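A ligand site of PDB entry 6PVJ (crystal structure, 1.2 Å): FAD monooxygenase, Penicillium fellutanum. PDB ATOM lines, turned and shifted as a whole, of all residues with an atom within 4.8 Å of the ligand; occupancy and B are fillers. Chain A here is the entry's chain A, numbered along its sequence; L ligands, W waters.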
ATOM      1  N   VAL A  13      10.370 -18.304  10.636  1.00  0.00           N
ATOM      2  CA  VAL A  13      10.773 -19.472  11.418  1.00  0.00           C
ATOM      3  C   VAL A  13       9.969 -19.487  12.707  1.00  0.00           C
ATOM      4  O   VAL A  13      10.223 -18.694  13.633  1.00  0.00           O
ATOM      5  CB  VAL A  13      12.272 -19.455  11.727  1.00  0.00           C
ATOM      6  CG1 VAL A  13      12.659 -20.694  12.521  1.00  0.00           C
ATOM      7  CG2 VAL A  13      13.086 -19.347  10.431  1.00  0.00           C
ATOM      8  N   GLY A  14       9.009 -20.411  12.791  1.00  0.00           N
ATOM      9  CA  GLY A  14       8.182 -20.587  13.968  1.00  0.00           C
ATOM     10  C   GLY A  14       6.801 -19.969  13.796  1.00  0.00           C
ATOM     11  O   GLY A  14       6.683 -18.763  13.512  1.00  0.00           O
ATOM     12  N   LEU A  15       5.766 -20.782  13.976  1.00  0.00           N
ATOM     13  CA  LEU A  15       4.380 -20.349  13.880  1.00  0.00           C
ATOM     14  C   LEU A  15       3.659 -20.471  15.221  1.00  0.00           C
ATOM     15  O   LEU A  15       2.635 -21.159  15.334  1.00  0.00           O
ATOM     16  CB  LEU A  15       3.649 -21.081  12.753  1.00  0.00           C
ATOM     17  CG  LEU A  15       4.076 -20.699  11.327  1.00  0.00           C
ATOM     18  CD1 LEU A  15       3.335 -21.526  10.288  1.00  0.00           C
ATOM     19  CD2 LEU A  15       3.845 -19.196  11.070  1.00  0.00           C
ATOM     20  N   GLY A  16       4.197 -19.815  16.246  1.00  0.00           N
ATOM     21  CA  GLY A  16       3.410 -19.434  17.393  1.00  0.00           C
ATOM     22  C   GLY A  16       2.552 -18.233  17.031  1.00  0.00           C
ATOM     23  O   GLY A  16       2.321 -17.930  15.858  1.00  0.00           O
ATOM     24  N   ILE A  17       2.088 -17.524  18.063  1.00  0.00           N
ATOM     25  CA  ILE A  17       1.217 -16.383  17.823  1.00  0.00           C
ATOM     26  C   ILE A  17       1.942 -15.326  16.987  1.00  0.00           C
ATOM     27  O   ILE A  17       1.351 -14.742  16.067  1.00  0.00           O
ATOM     28  CB  ILE A  17       0.744 -15.800  19.167  1.00  0.00           C
ATOM     29  CG1 ILE A  17      -0.093 -16.842  19.909  1.00  0.00           C
ATOM     30  CG2 ILE A  17      -0.039 -14.505  18.932  1.00  0.00           C
ATOM     31  CD1 ILE A  17      -0.469 -16.381  21.292  1.00  0.00           C
ATOM     32  N   VAL A  18       3.218 -15.093  17.290  1.00  0.00           N
ATOM     33  CA  VAL A  18       3.935 -13.988  16.661  1.00  0.00           C
ATOM     34  C   VAL A  18       4.268 -14.316  15.210  1.00  0.00           C
ATOM     35  O   VAL A  18       4.117 -13.462  14.320  1.00  0.00           O
ATOM     36  CB  VAL A  18       5.156 -13.593  17.498  1.00  0.00           C
ATOM     37  CG1 VAL A  18       5.974 -12.521  16.778  1.00  0.00           C
ATOM     38  CG2 VAL A  18       4.690 -13.098  18.863  1.00  0.00           C
ATOM     39  N   GLY A  19       4.736 -15.535  14.940  1.00  0.00           N
ATOM     40  CA  GLY A  19       5.018 -15.918  13.569  1.00  0.00           C
ATOM     41  C   GLY A  19       3.776 -15.887  12.701  1.00  0.00           C
ATOM     42  O   GLY A  19       3.826 -15.475  11.543  1.00  0.00           O
ATOM     43  N   PHE A  36       7.734 -21.667   8.259  1.00  0.00           N
ATOM     44  CA  PHE A  36       8.150 -23.016   8.626  1.00  0.00           C
ATOM     45  C   PHE A  36       7.923 -23.220  10.111  1.00  0.00           C
ATOM     46  O   PHE A  36       8.143 -22.324  10.918  1.00  0.00           O
ATOM     47  CB  PHE A  36       9.624 -23.203   8.326  1.00  0.00           C
ATOM     48  CG  PHE A  36       9.951 -23.071   6.871  1.00  0.00           C
ATOM     49  CD1 PHE A  36       9.889 -24.177   6.039  1.00  0.00           C
ATOM     50  CD2 PHE A  36      10.274 -21.837   6.325  1.00  0.00           C
ATOM     51  CE1 PHE A  36      10.172 -24.067   4.695  1.00  0.00           C
ATOM     52  CE2 PHE A  36      10.534 -21.719   4.976  1.00  0.00           C
ATOM     53  CZ  PHE A  36      10.495 -22.843   4.153  1.00  0.00           C
ATOM     54  N   GLU A  37       7.519 -24.439  10.478  1.00  0.00           N
ATOM     55  CA  GLU A  37       7.162 -24.730  11.858  1.00  0.00           C
ATOM     56  C   GLU A  37       7.415 -26.213  12.109  1.00  0.00           C
ATOM     57  O   GLU A  37       7.014 -27.062  11.297  1.00  0.00           O
ATOM     58  CB  GLU A  37       5.684 -24.402  12.105  1.00  0.00           C
ATOM     59  CG  GLU A  37       5.059 -25.053  13.319  1.00  0.00           C
ATOM     60  CD  GLU A  37       5.696 -24.635  14.638  1.00  0.00           C
ATOM     61  OE1 GLU A  37       5.798 -23.430  14.920  1.00  0.00           O
ATOM     62  OE2 GLU A  37       6.092 -25.534  15.422  1.00  0.00           O
ATOM     63  N   LYS A  38       8.069 -26.516  13.227  1.00  0.00           N
ATOM     64  CA  LYS A  38       8.493 -27.885  13.459  1.00  0.00           C
ATOM     65  C   LYS A  38       7.382 -28.817  13.920  1.00  0.00           C
ATOM     66  O   LYS A  38       7.487 -30.028  13.721  1.00  0.00           O
ATOM     67  CB  LYS A  38       9.683 -27.936  14.418  1.00  0.00           C
ATOM     68  CG  LYS A  38       9.395 -27.492  15.837  1.00  0.00           C
ATOM     69  CD  LYS A  38      10.705 -27.452  16.634  1.00  0.00           C
ATOM     70  CE  LYS A  38      10.494 -27.784  18.093  1.00  0.00           C
ATOM     71  NZ  LYS A  38       9.439 -26.962  18.732  1.00  0.00           N
ATOM     72  N   SER A  39       6.314 -28.290  14.519  1.00  0.00           N
ATOM     73  CA  SER A  39       5.336 -29.125  15.196  1.00  0.00           C
ATOM     74  C   SER A  39       3.936 -28.936  14.607  1.00  0.00           C
ATOM     75  O   SER A  39       3.661 -27.986  13.864  1.00  0.00           O
ATOM     76  CB  SER A  39       5.325 -28.843  16.704  1.00  0.00           C
ATOM     77  OG  SER A  39       4.691 -27.612  16.987  1.00  0.00           O
ATOM     78  N   ILE A  41       1.018 -27.378  15.215  1.00  0.00           N
ATOM     79  CA  ILE A  41       0.625 -26.282  16.108  1.00  0.00           C
ATOM     80  C   ILE A  41      -0.856 -26.262  16.419  1.00  0.00           C
ATOM     81  O   ILE A  41      -1.279 -25.466  17.257  1.00  0.00           O
ATOM     82  CB  ILE A  41       1.052 -24.934  15.516  1.00  0.00           C
ATOM     83  CG1 ILE A  41       0.573 -24.793  14.053  1.00  0.00           C
ATOM     84  CG2 ILE A  41       2.528 -24.785  15.643  1.00  0.00           C
ATOM     85  CD1 ILE A  41       0.670 -23.381  13.482  1.00  0.00           C
ATOM     86  N   ILE A  45      -2.923 -27.588  23.552  1.00  0.00           N
ATOM     87  CA  ILE A  45      -1.891 -27.487  24.582  1.00  0.00           C
ATOM     88  C   ILE A  45      -1.951 -26.080  25.174  1.00  0.00           C
ATOM     89  O   ILE A  45      -2.319 -25.119  24.493  1.00  0.00           O
ATOM     90  CB  ILE A  45      -0.508 -27.818  23.971  1.00  0.00           C
ATOM     91  CG1 ILE A  45       0.582 -27.770  25.054  1.00  0.00           C
ATOM     92  CG2 ILE A  45      -0.193 -26.886  22.812  1.00  0.00           C
ATOM     93  CD1 ILE A  45       1.866 -28.380  24.587  1.00  0.00           C
ATOM     94  N   GLY A  46      -1.622 -25.965  26.452  1.00  0.00           N
ATOM     95  CA  GLY A  46      -1.636 -24.679  27.118  1.00  0.00           C
ATOM     96  C   GLY A  46      -3.020 -24.319  27.636  1.00  0.00           C
ATOM     97  O   GLY A  46      -3.933 -25.145  27.694  1.00  0.00           O
ATOM     98  N   ASP A  47      -3.164 -23.050  28.017  1.00  0.00           N
ATOM     99  CA  ASP A  47      -4.449 -22.564  28.521  1.00  0.00           C
ATOM    100  C   ASP A  47      -4.896 -21.323  27.766  1.00  0.00           C
ATOM    101  O   ASP A  47      -4.949 -21.362  26.530  1.00  0.00           O
ATOM    102  CB  ASP A  47      -4.506 -22.504  30.069  1.00  0.00           C
ATOM    103  CG  ASP A  47      -3.534 -21.512  30.689  1.00  0.00           C
ATOM    104  OD1 ASP A  47      -3.927 -20.339  30.862  1.00  0.00           O
ATOM    105  OD2 ASP A  47      -2.400 -21.908  31.063  1.00  0.00           O
ATOM    106  N   CYS A  48      -5.257 -20.232  28.447  1.00  0.00           N
ATOM    107  CA  CYS A  48      -5.774 -19.044  27.779  1.00  0.00           C
ATOM    108  C   CYS A  48      -4.708 -17.977  27.590  1.00  0.00           C
ATOM    109  O   CYS A  48      -3.794 -17.817  28.416  1.00  0.00           O
ATOM    110  CB  CYS A  48      -6.960 -18.436  28.541  1.00  0.00           C
ATOM    111  SG  CYS A  48      -8.470 -19.326  28.303  1.00  0.00           S
ATOM    112  N   ILE A  49      -4.820 -17.256  26.465  1.00  0.00           N
ATOM    113  CA  ILE A  49      -4.005 -16.106  26.113  1.00  0.00           C
ATOM    114  C   ILE A  49      -4.894 -14.881  26.176  1.00  0.00           C
ATOM    115  O   ILE A  49      -6.063 -14.934  25.752  1.00  0.00           O
ATOM    116  CB  ILE A  49      -3.478 -16.260  24.655  1.00  0.00           C
ATOM    117  CG1 ILE A  49      -2.414 -17.356  24.554  1.00  0.00           C
ATOM    118  CG2 ILE A  49      -2.957 -14.926  24.107  1.00  0.00           C
ATOM    119  CD1 ILE A  49      -1.031 -16.895  24.939  1.00  0.00           C
ATOM    120  N   ARG A 109      -5.214 -20.567  23.831  1.00  0.00           N
ATOM    121  CA  ARG A 109      -4.158 -20.378  22.836  1.00  0.00           C
ATOM    122  C   ARG A 109      -4.418 -21.219  21.593  1.00  0.00           C
ATOM    123  O   ARG A 109      -4.215 -20.747  20.469  1.00  0.00           O
ATOM    124  CB  ARG A 109      -2.795 -20.742  23.418  1.00  0.00           C
ATOM    125  CG  ARG A 109      -1.633 -20.460  22.466  1.00  0.00           C
ATOM    126  CD  ARG A 109      -0.331 -20.843  23.142  1.00  0.00           C
ATOM    127  NE  ARG A 109       0.833 -20.617  22.293  1.00  0.00           N
ATOM    128  CZ  ARG A 109       1.258 -21.447  21.339  1.00  0.00           C
ATOM    129  NH1 ARG A 109       0.601 -22.561  21.078  1.00  0.00           N
ATOM    130  NH2 ARG A 109       2.354 -21.152  20.647  1.00  0.00           N
ATOM    131  N   VAL A 131       8.845 -29.000   9.830  1.00  0.00           N
ATOM    132  CA  VAL A 131      10.150 -28.521   9.378  1.00  0.00           C
ATOM    133  C   VAL A 131      10.870 -27.885  10.562  1.00  0.00           C
ATOM    134  O   VAL A 131      10.380 -26.919  11.152  1.00  0.00           O
ATOM    135  CB  VAL A 131      10.037 -27.525   8.215  1.00  0.00           C
ATOM    136  CG1 VAL A 131      11.412 -26.957   7.906  1.00  0.00           C
ATOM    137  CG2 VAL A 131       9.450 -28.184   6.991  1.00  0.00           C
ATOM    138  N   GLU A 132      12.055 -28.405  10.889  1.00  0.00           N
ATOM    139  CA  GLU A 132      12.965 -27.777  11.848  1.00  0.00           C
ATOM    140  C   GLU A 132      13.921 -26.912  11.028  1.00  0.00           C
ATOM    141  O   GLU A 132      14.715 -27.434  10.238  1.00  0.00           O
ATOM    142  CB  GLU A 132      13.732 -28.847  12.610  1.00  0.00           C
ATOM    143  CG  GLU A 132      14.801 -28.284  13.556  1.00  0.00           C
ATOM    144  CD  GLU A 132      15.639 -29.348  14.248  1.00  0.00           C
ATOM    145  OE1 GLU A 132      15.348 -30.553  14.089  1.00  0.00           O
ATOM    146  OE2 GLU A 132      16.592 -28.971  14.970  1.00  0.00           O
ATOM    147  N   VAL A 133      13.852 -25.592  11.202  1.00  0.00           N
ATOM    148  CA  VAL A 133      14.739 -24.687  10.493  1.00  0.00           C
ATOM    149  C   VAL A 133      16.068 -24.619  11.223  1.00  0.00           C
ATOM    150  O   VAL A 133      16.111 -24.446  12.445  1.00  0.00           O
ATOM    151  CB  VAL A 133      14.108 -23.296  10.359  1.00  0.00           C
ATOM    152  CG1 VAL A 133      15.078 -22.363   9.658  1.00  0.00           C
ATOM    153  CG2 VAL A 133      12.821 -23.391   9.609  1.00  0.00           C
ATOM    154  N   SER A 165      10.874 -16.042  14.655  1.00  0.00           N
ATOM    155  CA  SER A 165       9.775 -16.022  15.610  1.00  0.00           C
ATOM    156  C   SER A 165       9.666 -17.380  16.293  1.00  0.00           C
ATOM    157  O   SER A 165       8.568 -17.945  16.427  1.00  0.00           O
ATOM    158  CB  SER A 165       8.476 -15.598  14.928  1.00  0.00           C
ATOM    159  OG  SER A 165       8.245 -16.291  13.706  1.00  0.00           O
ATOM    160  N   ASP A 166      10.801 -17.908  16.741  1.00  0.00           N
ATOM    161  CA  ASP A 166      10.887 -19.279  17.212  1.00  0.00           C
ATOM    162  C   ASP A 166      10.852 -19.398  18.738  1.00  0.00           C
ATOM    163  O   ASP A 166      11.194 -20.456  19.282  1.00  0.00           O
ATOM    164  CB  ASP A 166      12.069 -20.025  16.566  1.00  0.00           C
ATOM    165  CG  ASP A 166      13.399 -19.315  16.712  1.00  0.00           C
ATOM    166  OD1 ASP A 166      13.467 -18.081  16.904  1.00  0.00           O
ATOM    167  OD2 ASP A 166      14.433 -20.011  16.594  1.00  0.00           O
ATOM    168  N   GLY A 167      10.394 -18.357  19.437  1.00  0.00           N
ATOM    169  CA  GLY A 167       9.971 -18.487  20.819  1.00  0.00           C
ATOM    170  C   GLY A 167      11.112 -18.374  21.817  1.00  0.00           C
ATOM    171  O   GLY A 167      12.257 -18.077  21.487  1.00  0.00           O
ATOM    172  N   VAL A 168      10.752 -18.599  23.090  1.00  0.00           N
ATOM    173  CA  VAL A 168      11.666 -18.339  24.205  1.00  0.00           C
ATOM    174  C   VAL A 168      12.951 -19.153  24.100  1.00  0.00           C
ATOM    175  O   VAL A 168      14.023 -18.694  24.524  1.00  0.00           O
ATOM    176  CB  VAL A 168      10.939 -18.533  25.553  1.00  0.00           C
ATOM    177  CG1 VAL A 168      10.481 -19.986  25.733  1.00  0.00           C
ATOM    178  CG2 VAL A 168      11.842 -18.074  26.711  1.00  0.00           C
ATOM    179  N   MET A 172      17.509 -19.710  16.568  1.00  0.00           N
ATOM    180  CA  MET A 172      17.932 -18.647  15.657  1.00  0.00           C
ATOM    181  C   MET A 172      18.666 -17.528  16.397  1.00  0.00           C
ATOM    182  O   MET A 172      19.507 -16.836  15.804  1.00  0.00           O
ATOM    183  CB  MET A 172      16.724 -18.066  14.906  1.00  0.00           C
ATOM    184  CG  MET A 172      15.960 -19.029  14.014  1.00  0.00           C
ATOM    185  SD  MET A 172      16.910 -19.727  12.648  1.00  0.00           S
ATOM    186  CE  MET A 172      17.305 -21.345  13.320  1.00  0.00           C
ATOM    187  N   ARG A 192      -1.330 -23.188  36.427  1.00  0.00           N
ATOM    188  CA  ARG A 192      -2.347 -22.633  35.540  1.00  0.00           C
ATOM    189  C   ARG A 192      -2.890 -23.702  34.611  1.00  0.00           C
ATOM    190  O   ARG A 192      -2.196 -24.660  34.251  1.00  0.00           O
ATOM    191  CB  ARG A 192      -1.827 -21.428  34.740  1.00  0.00           C
ATOM    192  CG  ARG A 192      -0.509 -21.625  34.035  1.00  0.00           C
ATOM    193  CD  ARG A 192      -0.015 -20.313  33.403  1.00  0.00           C
ATOM    194  NE  ARG A 192      -0.955 -19.831  32.380  1.00  0.00           N
ATOM    195  CZ  ARG A 192      -1.333 -18.573  32.218  1.00  0.00           C
ATOM    196  NH1 ARG A 192      -0.869 -17.601  33.011  1.00  0.00           N
ATOM    197  NH2 ARG A 192      -2.202 -18.264  31.267  1.00  0.00           N
ATOM    198  N   TRP A 256       5.609 -25.879  28.412  1.00  0.00           N
ATOM    199  CA  TRP A 256       4.182 -25.991  28.658  1.00  0.00           C
ATOM    200  C   TRP A 256       3.710 -27.445  28.669  1.00  0.00           C
ATOM    201  O   TRP A 256       2.502 -27.697  28.565  1.00  0.00           O
ATOM    202  CB  TRP A 256       3.410 -25.149  27.637  1.00  0.00           C
ATOM    203  CG  TRP A 256       3.679 -23.679  27.818  1.00  0.00           C
ATOM    204  CD1 TRP A 256       4.684 -22.945  27.239  1.00  0.00           C
ATOM    205  CD2 TRP A 256       2.952 -22.766  28.645  1.00  0.00           C
ATOM    206  NE1 TRP A 256       4.617 -21.636  27.662  1.00  0.00           N
ATOM    207  CE2 TRP A 256       3.553 -21.498  28.531  1.00  0.00           C
ATOM    208  CE3 TRP A 256       1.835 -22.902  29.471  1.00  0.00           C
ATOM    209  CZ2 TRP A 256       3.084 -20.380  29.204  1.00  0.00           C
ATOM    210  CZ3 TRP A 256       1.366 -21.785  30.145  1.00  0.00           C
ATOM    211  CH2 TRP A 256       1.987 -20.546  30.010  1.00  0.00           C
ATOM    212  N   ILE A 314      11.950 -11.536  16.676  1.00  0.00           N
ATOM    213  CA  ILE A 314      10.730 -10.907  17.187  1.00  0.00           C
ATOM    214  C   ILE A 314      10.027 -11.869  18.127  1.00  0.00           C
ATOM    215  O   ILE A 314      10.390 -13.045  18.252  1.00  0.00           O
ATOM    216  CB  ILE A 314       9.785 -10.418  16.070  1.00  0.00           C
ATOM    217  CG1 ILE A 314       9.246 -11.589  15.239  1.00  0.00           C
ATOM    218  CG2 ILE A 314      10.459  -9.368  15.166  1.00  0.00           C
ATOM    219  CD1 ILE A 314       8.103 -11.184  14.305  1.00  0.00           C
ATOM    220  N   GLY A 315       9.013 -11.353  18.834  1.00  0.00           N
ATOM    221  CA  GLY A 315       8.283 -12.188  19.772  1.00  0.00           C
ATOM    222  C   GLY A 315       9.143 -12.622  20.953  1.00  0.00           C
ATOM    223  O   GLY A 315      10.050 -11.904  21.396  1.00  0.00           O
ATOM    224  N   ASP A 316       8.875 -13.834  21.441  1.00  0.00           N
ATOM    225  CA  ASP A 316       9.586 -14.344  22.603  1.00  0.00           C
ATOM    226  C   ASP A 316      11.036 -14.676  22.290  1.00  0.00           C
ATOM    227  O   ASP A 316      11.831 -14.813  23.219  1.00  0.00           O
ATOM    228  CB  ASP A 316       8.887 -15.592  23.164  1.00  0.00           C
ATOM    229  CG  ASP A 316       7.652 -15.265  23.978  1.00  0.00           C
ATOM    230  OD1 ASP A 316       7.199 -14.095  23.979  1.00  0.00           O
ATOM    231  OD2 ASP A 316       7.129 -16.204  24.604  1.00  0.00           O
ATOM    232  N   ALA A 317      11.394 -14.841  21.008  1.00  0.00           N
ATOM    233  CA  ALA A 317      12.814 -14.972  20.664  1.00  0.00           C
ATOM    234  C   ALA A 317      13.581 -13.714  21.040  1.00  0.00           C
ATOM    235  O   ALA A 317      14.770 -13.804  21.370  1.00  0.00           O
ATOM    236  CB  ALA A 317      12.959 -15.257  19.165  1.00  0.00           C
ATOM    237  N   PRO A 323       3.990 -15.329  31.509  1.00  0.00           N
ATOM    238  CA  PRO A 323       2.540 -15.227  31.281  1.00  0.00           C
ATOM    239  C   PRO A 323       1.810 -14.394  32.317  1.00  0.00           C
ATOM    240  O   PRO A 323       0.645 -14.047  32.095  1.00  0.00           O
ATOM    241  CB  PRO A 323       2.077 -16.692  31.293  1.00  0.00           C
ATOM    242  CG  PRO A 323       3.110 -17.411  32.086  1.00  0.00           C
ATOM    243  CD  PRO A 323       4.417 -16.715  31.781  1.00  0.00           C
ATOM    244  N   ALA A 329       2.016 -11.695  24.441  1.00  0.00           N
ATOM    245  CA  ALA A 329       1.561 -11.902  23.072  1.00  0.00           C
ATOM    246  C   ALA A 329       1.340 -10.573  22.364  1.00  0.00           C
ATOM    247  O   ALA A 329       1.676 -10.418  21.188  1.00  0.00           O
ATOM    248  CB  ALA A 329       0.274 -12.719  23.064  1.00  0.00           C
HETATM  249  P1  LIG L   1       5.920 -19.335  20.740  1.00  0.00           P
HETATM  250  O1  LIG L   1       6.703 -20.024  21.765  1.00  0.00           O
HETATM  251  O2  LIG L   1       4.495 -19.179  20.983  1.00  0.00           O
HETATM  252  O3  LIG L   1       6.076 -20.068  19.414  1.00  0.00           O
HETATM  253  C1  LIG L   1       7.363 -20.466  18.885  1.00  0.00           C
HETATM  254  C2  LIG L   1       7.117 -21.476  17.785  1.00  0.00           C
HETATM  255  O4  LIG L   1       8.344 -21.707  17.054  1.00  0.00           O
HETATM  256  C3  LIG L   1       6.625 -22.851  18.254  1.00  0.00           C
HETATM  257  O5  LIG L   1       5.442 -23.253  17.566  1.00  0.00           O
HETATM  258  C4  LIG L   1       7.812 -23.788  17.974  1.00  0.00           C
HETATM  259  O6  LIG L   1       7.413 -25.116  17.644  1.00  0.00           O
HETATM  260  C5  LIG L   1       8.448 -23.090  16.771  1.00  0.00           C
HETATM  261  N1  LIG L   1       9.853 -23.406  16.531  1.00  0.00           N
HETATM  262  C6  LIG L   1      10.871 -23.268  17.435  1.00  0.00           C
HETATM  263  N2  LIG L   1      12.058 -23.548  16.941  1.00  0.00           N
HETATM  264  C7  LIG L   1      11.801 -23.835  15.604  1.00  0.00           C
HETATM  265  C8  LIG L   1      12.646 -24.184  14.535  1.00  0.00           C
HETATM  266  N3  LIG L   1      13.981 -24.293  14.642  1.00  0.00           N
HETATM  267  N4  LIG L   1      12.067 -24.428  13.330  1.00  0.00           N
HETATM  268  C9  LIG L   1      10.745 -24.308  13.224  1.00  0.00           C
HETATM  269  N5  LIG L   1       9.854 -23.979  14.159  1.00  0.00           N
HETATM  270  C10 LIG L   1      10.443 -23.745  15.340  1.00  0.00           C
HETATM  271  N6  LIG L   1       1.309 -18.248  27.009  1.00  0.00           N
HETATM  272  C11 LIG L   1       0.263 -17.931  27.810  1.00  0.00           C
HETATM  273  O7  LIG L   1       0.125 -16.801  28.302  1.00  0.00           O
HETATM  274  N7  LIG L   1      -0.709 -18.879  28.084  1.00  0.00           N
HETATM  275  C12 LIG L   1      -0.713 -20.174  27.617  1.00  0.00           C
HETATM  276  O8  LIG L   1      -1.628 -20.929  27.941  1.00  0.00           O
HETATM  277  C13 LIG L   1       0.408 -20.508  26.766  1.00  0.00           C
HETATM  278  N8  LIG L   1       0.487 -21.730  26.290  1.00  0.00           N
HETATM  279  C14 LIG L   1       1.560 -22.031  25.471  1.00  0.00           C
HETATM  280  C15 LIG L   1       1.657 -23.311  24.928  1.00  0.00           C
HETATM  281  C16 LIG L   1       2.719 -23.659  24.097  1.00  0.00           C
HETATM  282  C17 LIG L   1       2.805 -25.054  23.535  1.00  0.00           C
HETATM  283  C18 LIG L   1       3.697 -22.706  23.783  1.00  0.00           C
HETATM  284  C19 LIG L   1       4.856 -23.053  22.895  1.00  0.00           C
HETATM  285  C20 LIG L   1       3.609 -21.428  24.322  1.00  0.00           C
HETATM  286  C21 LIG L   1       2.543 -21.082  25.144  1.00  0.00           C
HETATM  287  N9  LIG L   1       2.431 -19.797  25.703  1.00  0.00           N
HETATM  288  C22 LIG L   1       1.380 -19.476  26.516  1.00  0.00           C
HETATM  289  C23 LIG L   1       3.414 -18.754  25.398  1.00  0.00           C
HETATM  290  C24 LIG L   1       2.937 -17.809  24.294  1.00  0.00           C
HETATM  291  O9  LIG L   1       2.597 -18.523  23.107  1.00  0.00           O
HETATM  292  C25 LIG L   1       4.046 -16.823  23.917  1.00  0.00           C
HETATM  293  O10 LIG L   1       4.479 -16.226  25.131  1.00  0.00           O
HETATM  294  C26 LIG L   1       3.484 -15.748  22.988  1.00  0.00           C
HETATM  295  O11 LIG L   1       2.227 -16.229  22.517  1.00  0.00           O
HETATM  296  C27 LIG L   1       4.266 -15.308  21.774  1.00  0.00           C
HETATM  297  O12 LIG L   1       5.405 -16.166  21.590  1.00  0.00           O
HETATM  298  P2  LIG L   1       5.969 -16.496  20.174  1.00  0.00           P
HETATM  299  O13 LIG L   1       7.131 -15.551  19.965  1.00  0.00           O
HETATM  300  O14 LIG L   1       4.968 -16.599  19.166  1.00  0.00           O
HETATM  301  O15 LIG L   1       6.554 -17.922  20.471  1.00  0.00           O
HETATM  302  O   HOH W   1       5.826 -17.495  16.680  1.00  0.00           O
HETATM  303  O   HOH W   2       4.223 -16.425  28.489  1.00  0.00           O
HETATM  304  O   HOH W   3       8.305 -22.165  22.311  1.00  0.00           O
HETATM  305  O   HOH W   4       7.870 -18.718  23.880  1.00  0.00           O
HETATM  306  O   HOH W   5      -1.227 -15.072  29.865  1.00  0.00           O
HETATM  307  O   HOH W   6      14.698 -22.577  17.095  1.00  0.00           O
HETATM  308  O   HOH W   7       9.546 -15.636  18.816  1.00  0.00           O
HETATM  309  O   HOH W   8      14.484 -26.269  17.349  1.00  0.00           O
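The backbone NH (N) of Lys 38 is in hydrogen-bond range of a nitrogen (N5) of the ligand (3.2 Å). An oxygen (O6) of the ligand sits at hydrogen-bond distance from the side-chain carboxylate (OE2) of Glu 37 (2.6 Å). The guanidinium group of Arg 109 is in salt-bridge range of an oxygen (O2) of the ligand, at 2.9 Å. The backbone NH of Val 133 sits at hydrogen-bond distance from a nitrogen (N4) of the ligand (3.0 Å). N7 of the ligand lies within hydrogen-bond range of O of Cys 48 (3.3 Å). N of Ile 17 sits at hydrogen-bond distance from O14 of the ligand (3.2 Å). OD2 of Asp 316 is in hydrogen-bond range of O10 of the ligand (2.7 Å). O14 of the ligand lies within hydrogen-bond range of N of Val 18 (3.0 Å). A nitrogen (N3) of the ligand is in hydrogen-bond range of the backbone carbonyl oxygen of Val 133. O8 of the ligand is in hydrogen-bond range of N of Asp 47, 2.6 Å away. The backbone NH of Asp 316 is in hydrogen-bond range of an oxygen (O13) of the ligand (2.9 Å). NZ of Lys 38 sits at hydrogen-bond distance from O6 of the ligand (2.9 Å).
Water W5 bridges O7 of the ligand (2.7 Å) and O of Pro 323 (3.1 Å). Water W4 lies within hydrogen-bond range of OD2 of Asp 316, O1 of the ligand and N of Val 168. Water W1 lies within hydrogen-bond range of O14 of the ligand, O of Ser 165, N of Gly 19 and N of Gly 16. Water W6 lies within hydrogen-bond range of OD2 of Asp 166 (2.6 Å) and N2 of the ligand (2.8 Å).
The backbone carbonyl oxygen (O) of Glu 37 is in hydrogen-bond range of the backbone NH (N) of Val 131, 3.0 Å away. N of Lys 38 is in hydrogen-bond range of O of Val 131. N of Asp 166 is in hydrogen-bond range of O of Val 13. The side-chain carboxylate of Glu 37 lies within hydrogen-bond range of the backbone NH of Leu 15 (2.8 Å). The guanidinium group (NH2) of Arg 192 is in salt-bridge range of the side-chain carboxylate (OD1) of Asp 47 (2.7 Å). O of Gly 14 lies within hydrogen-bond range of OG of Ser 165, at 2.9 Å. The backbone carbonyl oxygen (O) of Gly 167 sits close to the backbone NH (N) of Ala 317. The backbone NH (N) of Gly 14 sits at hydrogen-bond distance from the backbone carbonyl oxygen (O) of Phe 36 (2.8 Å).
The indole nitrogen (NE1) of Trp 256 lies close to a nitrogen (N9) of the ligand, 3.5 Å away. Merely in contact with the ligand: Val 13 (3.9 Å), Gly 14 (3.3 Å), Gly 16 (3.4 Å), Ser 39 (3.8 Å), Ile 41 (3.8 Å), Ile 45 (3.6 Å), Gly 46 (3.7 Å), Ile 49 (3.3 Å), Val 131 (3.4 Å), Glu 132 (3.8 Å), Ser 165 (3.7 Å), Asp 166 (3.4 Å), Gly 167 (3.5 Å), Arg 192 (3.6 Å), Gly 315 (3.6 Å) and Pro 323 (3.6 Å). Hydrophobic or aromatic side chains that line the ligand: Val 13, Ile 17, Val 18, Ile 41, Ile 45, Ile 49, Val 133, Trp 256 and Pro 323. Within 4 Å of the ligand: Val 13, Gly 14, Gly 16, Ile 17, Val 18, Glu 37, Lys 38, Ser 39, Ile 41, Ile 45, Gly 46, Asp 47, Cys 48, Ile 49, Arg 109, Val 131, Glu 132, Val 133, Ser 165, Asp 166, Gly 167, Arg 192, Trp 256, Gly 315, Asp 316 and Pro 323. The nearest printed residue that does not touch the ligand is Phe 36 (4.003 Å).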
